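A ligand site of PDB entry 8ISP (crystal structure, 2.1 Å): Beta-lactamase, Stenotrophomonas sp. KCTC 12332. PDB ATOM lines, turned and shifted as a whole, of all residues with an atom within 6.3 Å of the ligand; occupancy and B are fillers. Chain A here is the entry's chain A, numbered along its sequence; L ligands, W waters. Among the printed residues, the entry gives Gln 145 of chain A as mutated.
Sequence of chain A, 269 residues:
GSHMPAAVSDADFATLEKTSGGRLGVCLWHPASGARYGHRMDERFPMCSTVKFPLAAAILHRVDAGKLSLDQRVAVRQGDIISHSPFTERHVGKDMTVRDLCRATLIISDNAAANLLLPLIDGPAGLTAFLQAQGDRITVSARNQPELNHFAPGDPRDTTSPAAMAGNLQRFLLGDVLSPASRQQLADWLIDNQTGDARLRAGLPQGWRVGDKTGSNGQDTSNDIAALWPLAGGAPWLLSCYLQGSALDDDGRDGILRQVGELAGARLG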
ATOM      1  N   MET A  47       8.218 -31.361  -8.919  1.00  0.00           N
ATOM      2  CA  MET A  47       9.056 -31.976  -7.887  1.00  0.00           C
ATOM      3  C   MET A  47       9.772 -30.928  -7.045  1.00  0.00           C
ATOM      4  O   MET A  47       9.826 -31.030  -5.810  1.00  0.00           O
ATOM      5  CB  MET A  47      10.065 -32.927  -8.515  1.00  0.00           C
ATOM      6  CG  MET A  47       9.546 -34.322  -8.755  1.00  0.00           C
ATOM      7  SD  MET A  47      10.832 -35.436  -9.343  1.00  0.00           S
ATOM      8  CE  MET A  47      11.063 -34.847 -11.017  1.00  0.00           C
ATOM      9  N   CYS A  48      10.323 -29.903  -7.698  1.00  0.00           N
ATOM     10  CA  CYS A  48      11.223 -28.943  -7.060  1.00  0.00           C
ATOM     11  C   CYS A  48      12.391 -29.751  -6.468  1.00  0.00           C
ATOM     12  O   CYS A  48      12.866 -30.700  -7.113  1.00  0.00           O
ATOM     13  CB  CYS A  48      10.489 -28.082  -6.051  1.00  0.00           C
ATOM     14  SG  CYS A  48       9.182 -27.017  -6.722  1.00  0.00           S
ATOM     15  N   SER A  49      12.838 -29.435  -5.257  1.00  0.00           N
ATOM     16  CA  SER A  49      14.002 -30.084  -4.683  1.00  0.00           C
ATOM     17  C   SER A  49      13.764 -31.537  -4.299  1.00  0.00           C
ATOM     18  O   SER A  49      14.721 -32.243  -3.989  1.00  0.00           O
ATOM     19  CB  SER A  49      14.491 -29.301  -3.462  1.00  0.00           C
ATOM     20  OG  SER A  49      15.235 -28.180  -3.881  1.00  0.00           O
ATOM     21  N   THR A  50      12.511 -32.008  -4.306  1.00  0.00           N
ATOM     22  CA  THR A  50      12.282 -33.416  -3.980  1.00  0.00           C
ATOM     23  C   THR A  50      12.874 -34.359  -5.022  1.00  0.00           C
ATOM     24  O   THR A  50      13.013 -35.557  -4.748  1.00  0.00           O
ATOM     25  CB  THR A  50      10.794 -33.700  -3.799  1.00  0.00           C
ATOM     26  OG1 THR A  50      10.106 -33.548  -5.050  1.00  0.00           O
ATOM     27  CG2 THR A  50      10.187 -32.751  -2.772  1.00  0.00           C
ATOM     28  N   LYS A  52      15.807 -34.480  -5.628  1.00  0.00           N
ATOM     29  CA  LYS A  52      17.107 -34.878  -5.101  1.00  0.00           C
ATOM     30  C   LYS A  52      17.060 -36.233  -4.406  1.00  0.00           C
ATOM     31  O   LYS A  52      18.104 -36.853  -4.227  1.00  0.00           O
ATOM     32  CB  LYS A  52      17.624 -33.800  -4.140  1.00  0.00           C
ATOM     33  CG  LYS A  52      17.892 -32.465  -4.820  1.00  0.00           C
ATOM     34  CD  LYS A  52      17.967 -31.324  -3.818  1.00  0.00           C
ATOM     35  CE  LYS A  52      18.324 -30.003  -4.490  1.00  0.00           C
ATOM     36  NZ  LYS A  52      18.430 -28.901  -3.497  1.00  0.00           N
ATOM     37  N   SER A  83      22.587 -20.083  -6.289  1.00  0.00           N
ATOM     38  CA  SER A  83      21.969 -19.703  -5.025  1.00  0.00           C
ATOM     39  C   SER A  83      21.672 -20.937  -4.172  1.00  0.00           C
ATOM     40  O   SER A  83      21.392 -22.020  -4.677  1.00  0.00           O
ATOM     41  CB  SER A  83      20.681 -18.926  -5.268  1.00  0.00           C
ATOM     42  OG  SER A  83      20.926 -17.778  -6.067  1.00  0.00           O
ATOM     43  N   HIS A  84      21.770 -20.748  -2.855  1.00  0.00           N
ATOM     44  CA  HIS A  84      21.393 -21.757  -1.860  1.00  0.00           C
ATOM     45  C   HIS A  84      22.231 -23.031  -2.021  1.00  0.00           C
ATOM     46  O   HIS A  84      21.709 -24.139  -2.209  1.00  0.00           O
ATOM     47  CB  HIS A  84      19.886 -22.057  -1.935  1.00  0.00           C
ATOM     48  CG  HIS A  84      19.343 -22.686  -0.690  1.00  0.00           C
ATOM     49  ND1 HIS A  84      19.635 -23.989  -0.330  1.00  0.00           N
ATOM     50  CD2 HIS A  84      18.525 -22.204   0.267  1.00  0.00           C
ATOM     51  CE1 HIS A  84      19.014 -24.271   0.802  1.00  0.00           C
ATOM     52  NE2 HIS A  84      18.328 -23.212   1.188  1.00  0.00           N
ATOM     53  N   ILE A 108      20.391 -30.333   3.532  1.00  0.00           N
ATOM     54  CA  ILE A 108      20.253 -28.879   3.475  1.00  0.00           C
ATOM     55  C   ILE A 108      19.802 -28.391   2.105  1.00  0.00           C
ATOM     56  O   ILE A 108      19.625 -27.183   1.922  1.00  0.00           O
ATOM     57  CB  ILE A 108      21.569 -28.172   3.890  1.00  0.00           C
ATOM     58  CG1 ILE A 108      21.294 -26.777   4.453  1.00  0.00           C
ATOM     59  CG2 ILE A 108      22.537 -28.096   2.721  1.00  0.00           C
ATOM     60  CD1 ILE A 108      20.472 -26.770   5.719  1.00  0.00           C
ATOM     61  N   SER A 109      19.600 -29.294   1.146  1.00  0.00           N
ATOM     62  CA  SER A 109      19.168 -28.949  -0.206  1.00  0.00           C
ATOM     63  C   SER A 109      20.169 -28.004  -0.873  1.00  0.00           C
ATOM     64  O   SER A 109      19.820 -26.913  -1.335  1.00  0.00           O
ATOM     65  CB  SER A 109      17.742 -28.375  -0.185  1.00  0.00           C
ATOM     66  OG  SER A 109      17.042 -28.687  -1.370  1.00  0.00           O
ATOM     67  N   ASP A 110      21.422 -28.447  -0.903  1.00  0.00           N
ATOM     68  CA  ASP A 110      22.472 -27.746  -1.640  1.00  0.00           C
ATOM     69  C   ASP A 110      22.187 -27.862  -3.134  1.00  0.00           C
ATOM     70  O   ASP A 110      22.202 -28.957  -3.692  1.00  0.00           O
ATOM     71  CB  ASP A 110      23.836 -28.358  -1.301  1.00  0.00           C
ATOM     72  CG  ASP A 110      24.994 -27.508  -1.795  1.00  0.00           C
ATOM     73  OD1 ASP A 110      25.074 -27.236  -3.009  1.00  0.00           O
ATOM     74  OD2 ASP A 110      25.845 -27.121  -0.961  1.00  0.00           O
ATOM     75  N   ASN A 111      21.924 -26.710  -3.775  1.00  0.00           N
ATOM     76  CA  ASN A 111      21.501 -26.738  -5.170  1.00  0.00           C
ATOM     77  C   ASN A 111      22.654 -27.085  -6.106  1.00  0.00           C
ATOM     78  O   ASN A 111      22.475 -27.883  -7.040  1.00  0.00           O
ATOM     79  CB  ASN A 111      20.877 -25.394  -5.555  1.00  0.00           C
ATOM     80  CG  ASN A 111      19.457 -25.255  -5.057  1.00  0.00           C
ATOM     81  OD1 ASN A 111      18.747 -26.252  -4.872  1.00  0.00           O
ATOM     82  ND2 ASN A 111      19.032 -24.018  -4.832  1.00  0.00           N
ATOM     83  N   GLN A 145      19.230 -27.631 -11.783  1.00  0.00           N
ATOM     84  CA  GLN A 145      18.920 -26.427 -11.033  1.00  0.00           C
ATOM     85  C   GLN A 145      19.415 -25.187 -11.782  1.00  0.00           C
ATOM     86  O   GLN A 145      20.488 -25.238 -12.398  1.00  0.00           O
ATOM     87  CB  GLN A 145      19.534 -26.483  -9.638  1.00  0.00           C
ATOM     88  CG  GLN A 145      18.940 -27.546  -8.740  1.00  0.00           C
ATOM     89  CD  GLN A 145      17.622 -27.126  -8.119  1.00  0.00           C
ATOM     90  OE1 GLN A 145      16.849 -26.374  -8.711  1.00  0.00           O
ATOM     91  NE2 GLN A 145      17.352 -27.607  -6.905  1.00  0.00           N
ATOM     92  N   PRO A 146      18.690 -24.069 -11.716  1.00  0.00           N
ATOM     93  CA  PRO A 146      17.440 -23.912 -10.970  1.00  0.00           C
ATOM     94  C   PRO A 146      16.175 -24.069 -11.814  1.00  0.00           C
ATOM     95  O   PRO A 146      15.069 -23.991 -11.266  1.00  0.00           O
ATOM     96  CB  PRO A 146      17.555 -22.484 -10.440  1.00  0.00           C
ATOM     97  CG  PRO A 146      18.251 -21.767 -11.546  1.00  0.00           C
ATOM     98  CD  PRO A 146      19.178 -22.774 -12.212  1.00  0.00           C
ATOM     99  N   LEU A 148      14.608 -26.453 -13.069  1.00  0.00           N
ATOM    100  CA  LEU A 148      13.676 -27.554 -12.829  1.00  0.00           C
ATOM    101  C   LEU A 148      12.497 -27.115 -11.982  1.00  0.00           C
ATOM    102  O   LEU A 148      11.497 -27.841 -11.928  1.00  0.00           O
ATOM    103  CB  LEU A 148      14.397 -28.737 -12.182  1.00  0.00           C
ATOM    104  CG  LEU A 148      15.086 -28.601 -10.815  1.00  0.00           C
ATOM    105  CD1 LEU A 148      14.113 -28.831  -9.656  1.00  0.00           C
ATOM    106  CD2 LEU A 148      16.250 -29.567 -10.722  1.00  0.00           C
ATOM    107  N   ASN A 149      12.580 -25.955 -11.325  1.00  0.00           N
ATOM    108  CA  ASN A 149      11.447 -25.446 -10.566  1.00  0.00           C
ATOM    109  C   ASN A 149      10.342 -24.870 -11.447  1.00  0.00           C
ATOM    110  O   ASN A 149       9.257 -24.584 -10.938  1.00  0.00           O
ATOM    111  CB  ASN A 149      11.920 -24.381  -9.570  1.00  0.00           C
ATOM    112  CG  ASN A 149      12.499 -24.984  -8.314  1.00  0.00           C
ATOM    113  OD1 ASN A 149      11.823 -25.100  -7.300  1.00  0.00           O
ATOM    114  ND2 ASN A 149      13.773 -25.366  -8.381  1.00  0.00           N
ATOM    115  N   THR A 195      15.742 -29.239   6.859  1.00  0.00           N
ATOM    116  CA  THR A 195      14.818 -28.244   6.331  1.00  0.00           C
ATOM    117  C   THR A 195      13.354 -28.599   6.531  1.00  0.00           C
ATOM    118  O   THR A 195      12.486 -27.955   5.927  1.00  0.00           O
ATOM    119  CB  THR A 195      15.089 -28.031   4.831  1.00  0.00           C
ATOM    120  OG1 THR A 195      14.688 -29.212   4.109  1.00  0.00           O
ATOM    121  CG2 THR A 195      16.561 -27.768   4.596  1.00  0.00           C
ATOM    122  N   ARG A 199       7.446 -28.484   8.801  1.00  0.00           N
ATOM    123  CA  ARG A 199       6.602 -29.045   7.753  1.00  0.00           C
ATOM    124  C   ARG A 199       5.974 -30.328   8.302  1.00  0.00           C
ATOM    125  O   ARG A 199       5.318 -30.266   9.348  1.00  0.00           O
ATOM    126  CB  ARG A 199       7.383 -29.225   6.454  1.00  0.00           C
ATOM    127  CG  ARG A 199       7.627 -27.909   5.724  1.00  0.00           C
ATOM    128  CD  ARG A 199       8.934 -27.910   4.949  1.00  0.00           C
ATOM    129  NE  ARG A 199       9.017 -26.777   4.030  1.00  0.00           N
ATOM    130  CZ  ARG A 199      10.135 -26.317   3.487  1.00  0.00           C
ATOM    131  NH1 ARG A 199      11.303 -26.899   3.760  1.00  0.00           N
ATOM    132  NH2 ARG A 199      10.094 -25.277   2.667  1.00  0.00           N
ATOM    133  N   LYS A 213      12.562 -35.255   2.708  1.00  0.00           N
ATOM    134  CA  LYS A 213      13.182 -34.301   1.799  1.00  0.00           C
ATOM    135  C   LYS A 213      12.134 -33.303   1.346  1.00  0.00           C
ATOM    136  O   LYS A 213      11.002 -33.676   1.037  1.00  0.00           O
ATOM    137  CB  LYS A 213      13.787 -34.995   0.568  1.00  0.00           C
ATOM    138  CG  LYS A 213      14.459 -34.027  -0.410  1.00  0.00           C
ATOM    139  CD  LYS A 213      15.716 -33.420   0.188  1.00  0.00           C
ATOM    140  CE  LYS A 213      16.246 -32.263  -0.645  1.00  0.00           C
ATOM    141  NZ  LYS A 213      15.514 -30.985  -0.412  1.00  0.00           N
ATOM    142  N   THR A 214      12.518 -32.026   1.316  1.00  0.00           N
ATOM    143  CA  THR A 214      11.608 -30.923   1.065  1.00  0.00           C
ATOM    144  C   THR A 214      11.890 -30.282  -0.291  1.00  0.00           C
ATOM    145  O   THR A 214      12.830 -30.650  -1.006  1.00  0.00           O
ATOM    146  CB  THR A 214      11.704 -29.884   2.178  1.00  0.00           C
ATOM    147  OG1 THR A 214      13.046 -29.405   2.264  1.00  0.00           O
ATOM    148  CG2 THR A 214      11.310 -30.503   3.514  1.00  0.00           C
ATOM    149  N   GLY A 215      11.048 -29.319  -0.650  1.00  0.00           N
ATOM    150  CA  GLY A 215      11.199 -28.535  -1.864  1.00  0.00           C
ATOM    151  C   GLY A 215      10.306 -27.302  -1.843  1.00  0.00           C
ATOM    152  O   GLY A 215       9.242 -27.317  -1.222  1.00  0.00           O
ATOM    153  N   SER A 216      10.731 -26.231  -2.507  1.00  0.00           N
ATOM    154  CA  SER A 216       9.946 -24.999  -2.546  1.00  0.00           C
ATOM    155  C   SER A 216      10.429 -24.125  -3.695  1.00  0.00           C
ATOM    156  O   SER A 216      11.613 -24.144  -4.052  1.00  0.00           O
ATOM    157  CB  SER A 216      10.032 -24.223  -1.228  1.00  0.00           C
ATOM    158  OG  SER A 216       9.322 -22.994  -1.326  1.00  0.00           O
ATOM    159  N   ASN A 217       9.504 -23.355  -4.262  1.00  0.00           N
ATOM    160  CA  ASN A 217       9.831 -22.389  -5.303  1.00  0.00           C
ATOM    161  C   ASN A 217       9.852 -20.954  -4.792  1.00  0.00           C
ATOM    162  O   ASN A 217      10.167 -20.038  -5.559  1.00  0.00           O
ATOM    163  CB  ASN A 217       8.864 -22.524  -6.486  1.00  0.00           C
ATOM    164  CG  ASN A 217       7.482 -21.953  -6.188  1.00  0.00           C
ATOM    165  OD1 ASN A 217       7.051 -21.871  -5.033  1.00  0.00           O
ATOM    166  ND2 ASN A 217       6.770 -21.578  -7.241  1.00  0.00           N
ATOM    167  N   GLY A 218       9.531 -20.739  -3.518  1.00  0.00           N
ATOM    168  CA  GLY A 218       9.612 -19.425  -2.924  1.00  0.00           C
ATOM    169  C   GLY A 218       8.442 -18.508  -3.200  1.00  0.00           C
ATOM    170  O   GLY A 218       8.487 -17.336  -2.809  1.00  0.00           O
ATOM    171  N   ASN A 223       6.803 -28.728  -1.136  1.00  0.00           N
ATOM    172  CA  ASN A 223       6.650 -30.169  -1.125  1.00  0.00           C
ATOM    173  C   ASN A 223       7.438 -30.775   0.024  1.00  0.00           C
ATOM    174  O   ASN A 223       8.395 -30.180   0.542  1.00  0.00           O
ATOM    175  CB  ASN A 223       7.111 -30.792  -2.452  1.00  0.00           C
ATOM    176  CG  ASN A 223       6.544 -30.072  -3.664  1.00  0.00           C
ATOM    177  OD1 ASN A 223       5.369 -29.716  -3.692  1.00  0.00           O
ATOM    178  ND2 ASN A 223       7.391 -29.858  -4.663  1.00  0.00           N
ATOM    179  N   ASP A 250       5.569 -19.140   2.006  1.00  0.00           N
ATOM    180  CA  ASP A 250       6.307 -20.298   2.489  1.00  0.00           C
ATOM    181  C   ASP A 250       5.855 -20.700   3.892  1.00  0.00           C
ATOM    182  O   ASP A 250       5.695 -21.892   4.187  1.00  0.00           O
ATOM    183  CB  ASP A 250       7.806 -20.024   2.453  1.00  0.00           C
ATOM    184  CG  ASP A 250       8.424 -20.408   1.134  1.00  0.00           C
ATOM    185  OD1 ASP A 250       8.405 -19.570   0.208  1.00  0.00           O
ATOM    186  OD2 ASP A 250       8.907 -21.557   1.006  1.00  0.00           O
HETATM  187  C1  LIG L   1      14.412 -25.625  -0.393  1.00  0.00           C
HETATM  188  C2  LIG L   1      15.026 -23.688  -4.907  1.00  0.00           C
HETATM  189  C3  LIG L   1      14.408 -27.101  -3.690  1.00  0.00           C
HETATM  190  C4  LIG L   1      13.686 -23.562   0.843  1.00  0.00           C
HETATM  191  C5  LIG L   1      15.529 -20.796  -3.815  1.00  0.00           C
HETATM  192  C6  LIG L   1      16.095 -25.853  -2.378  1.00  0.00           C
HETATM  193  C7  LIG L   1      14.333 -21.457  -4.014  1.00  0.00           C
HETATM  194  C8  LIG L   1      13.268 -21.238  -3.169  1.00  0.00           C
HETATM  195  C9  LIG L   1      15.288 -23.376  -1.110  1.00  0.00           C
HETATM  196  C10 LIG L   1      13.385 -20.344  -2.116  1.00  0.00           C
HETATM  197  C11 LIG L   1      14.579 -24.314  -0.133  1.00  0.00           C
HETATM  198  C12 LIG L   1      14.587 -19.675  -1.907  1.00  0.00           C
HETATM  199  C13 LIG L   1      15.658 -19.905  -2.757  1.00  0.00           C
HETATM  200  C14 LIG L   1      14.194 -22.447  -5.177  1.00  0.00           C
HETATM  201  C15 LIG L   1      15.342 -25.892  -3.712  1.00  0.00           C
HETATM  202  C16 LIG L   1      13.654 -26.577   0.555  1.00  0.00           C
HETATM  203  N1  LIG L   1      14.627 -21.830  -6.418  1.00  0.00           N
HETATM  204  N2  LIG L   1      14.561 -24.698  -3.967  1.00  0.00           N
HETATM  205  N3  LIG L   1      15.248 -26.377  -1.317  1.00  0.00           N
HETATM  206  O1  LIG L   1      16.071 -23.833  -5.458  1.00  0.00           O
HETATM  207  O2  LIG L   1      13.230 -26.957  -3.773  1.00  0.00           O
HETATM  208  O3  LIG L   1      13.440 -27.754   0.157  1.00  0.00           O
HETATM  209  O4  LIG L   1      13.274 -26.280   1.717  1.00  0.00           O
HETATM  210  S1  LIG L   1      16.653 -24.186  -1.973  1.00  0.00           S
HETATM  211  O   HOH W   1      12.136 -20.666  -7.050  1.00  0.00           O
HETATM  212  O   HOH W   2      18.682 -18.933  -1.663  1.00  0.00           O
HETATM  213  O   HOH W   3      10.980 -22.534   2.411  1.00  0.00           O
HETATM  214  O   HOH W   4      17.279 -20.696  -6.586  1.00  0.00           O
HETATM  215  O   HOH W   5      18.203 -23.988  -7.683  1.00  0.00           O
HETATM  216  O   HOH W   6      14.688 -24.874   3.798  1.00  0.00           O
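O3 of the ligand lies within salt-bridge range of NZ of Lys 213.
O of Ser 216 is in hydrogen-bond range of N2 of the ligand.
An oxygen (O1) of the ligand is in hydrogen-bond range of the side-chain amide nitrogen of Asn 111, 3.0 Å away.
O2 of the ligand is in hydrogen-bond range of N of Ser 216 (2.9 Å).
The backbone NH of Gly 215 lies within hydrogen-bond range of an oxygen (O3) of the ligand.
The backbone NH (N) of Ser 49 lies close to an oxygen (O2) of the ligand (2.9 Å).
The side-chain hydroxyl (OG1) of Thr 214 lies within hydrogen-bond range of an oxygen (O3) of the ligand, at 2.7 Å.
The side-chain hydroxyl (OG) of Ser 49 is covalently linked to a carbon (C3) of the ligand.
ND1 of His 84 sits close to S1 of the ligand, at 3.4 Å.
An oxygen (O4) of the ligand is in salt-bridge range of the guanidinium group (NH1) of Arg 199 (2.9 Å).
The side-chain hydroxyl of Ser 109 is in hydrogen-bond range of a nitrogen (N3) of the ligand, 2.9 Å away.
Cys 48 touches the ligand.
Lys 52 touches the ligand.
Asn 217 touches the ligand (C to C8, 3.8 Å).
Gly 218 touches the ligand.
Of the 25 residues printed, 13 come within 4 Å of the ligand.
The nearest printed residue that does not touch the ligand is Thr 195 (4.01 Å).
Water W1 bridges O of Asn 217 and N1 of the ligand.
Water W5 lies within hydrogen-bond range of OE1 of Gln 145 (2.9 Å), ND2 of Asn 111 (3.0 Å) and O1 of the ligand (3.1 Å).
Water W3 lies within hydrogen-bond range of OD2 of Asp 250 (2.7 Å) and NH2 of Arg 199 (2.9 Å).
The guanidinium group (NH1) of Arg 199 is in hydrogen-bond range of the backbone carbonyl oxygen (O) of Thr 195 (2.7 Å).
OG of Ser 216 lies within hydrogen-bond range of OD2 of Asp 250 (2.8 Å).
The backbone NH (N) of Asn 111 is in hydrogen-bond range of the backbone carbonyl oxygen (O) of His 84 (3.0 Å).
The side-chain hydroxyl (OG1) of Thr 214 sits at hydrogen-bond distance from the guanidinium group (NH1) of Arg 199, at 3.4 Å.
NZ of Lys 213 is in hydrogen-bond range of OG of Ser 109.
The backbone carbonyl oxygen (O) of Ser 216 lies close to the side-chain amide oxygen (OD1) of Asn 149.
The side-chain amide oxygen (OD1) of Asn 111 sits at hydrogen-bond distance from the side-chain amino group (NZ) of Lys 52 (3.0 Å).
The side-chain hydroxyl (OG1) of Thr 195 is in hydrogen-bond range of the side-chain hydroxyl (OG1) of Thr 214.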
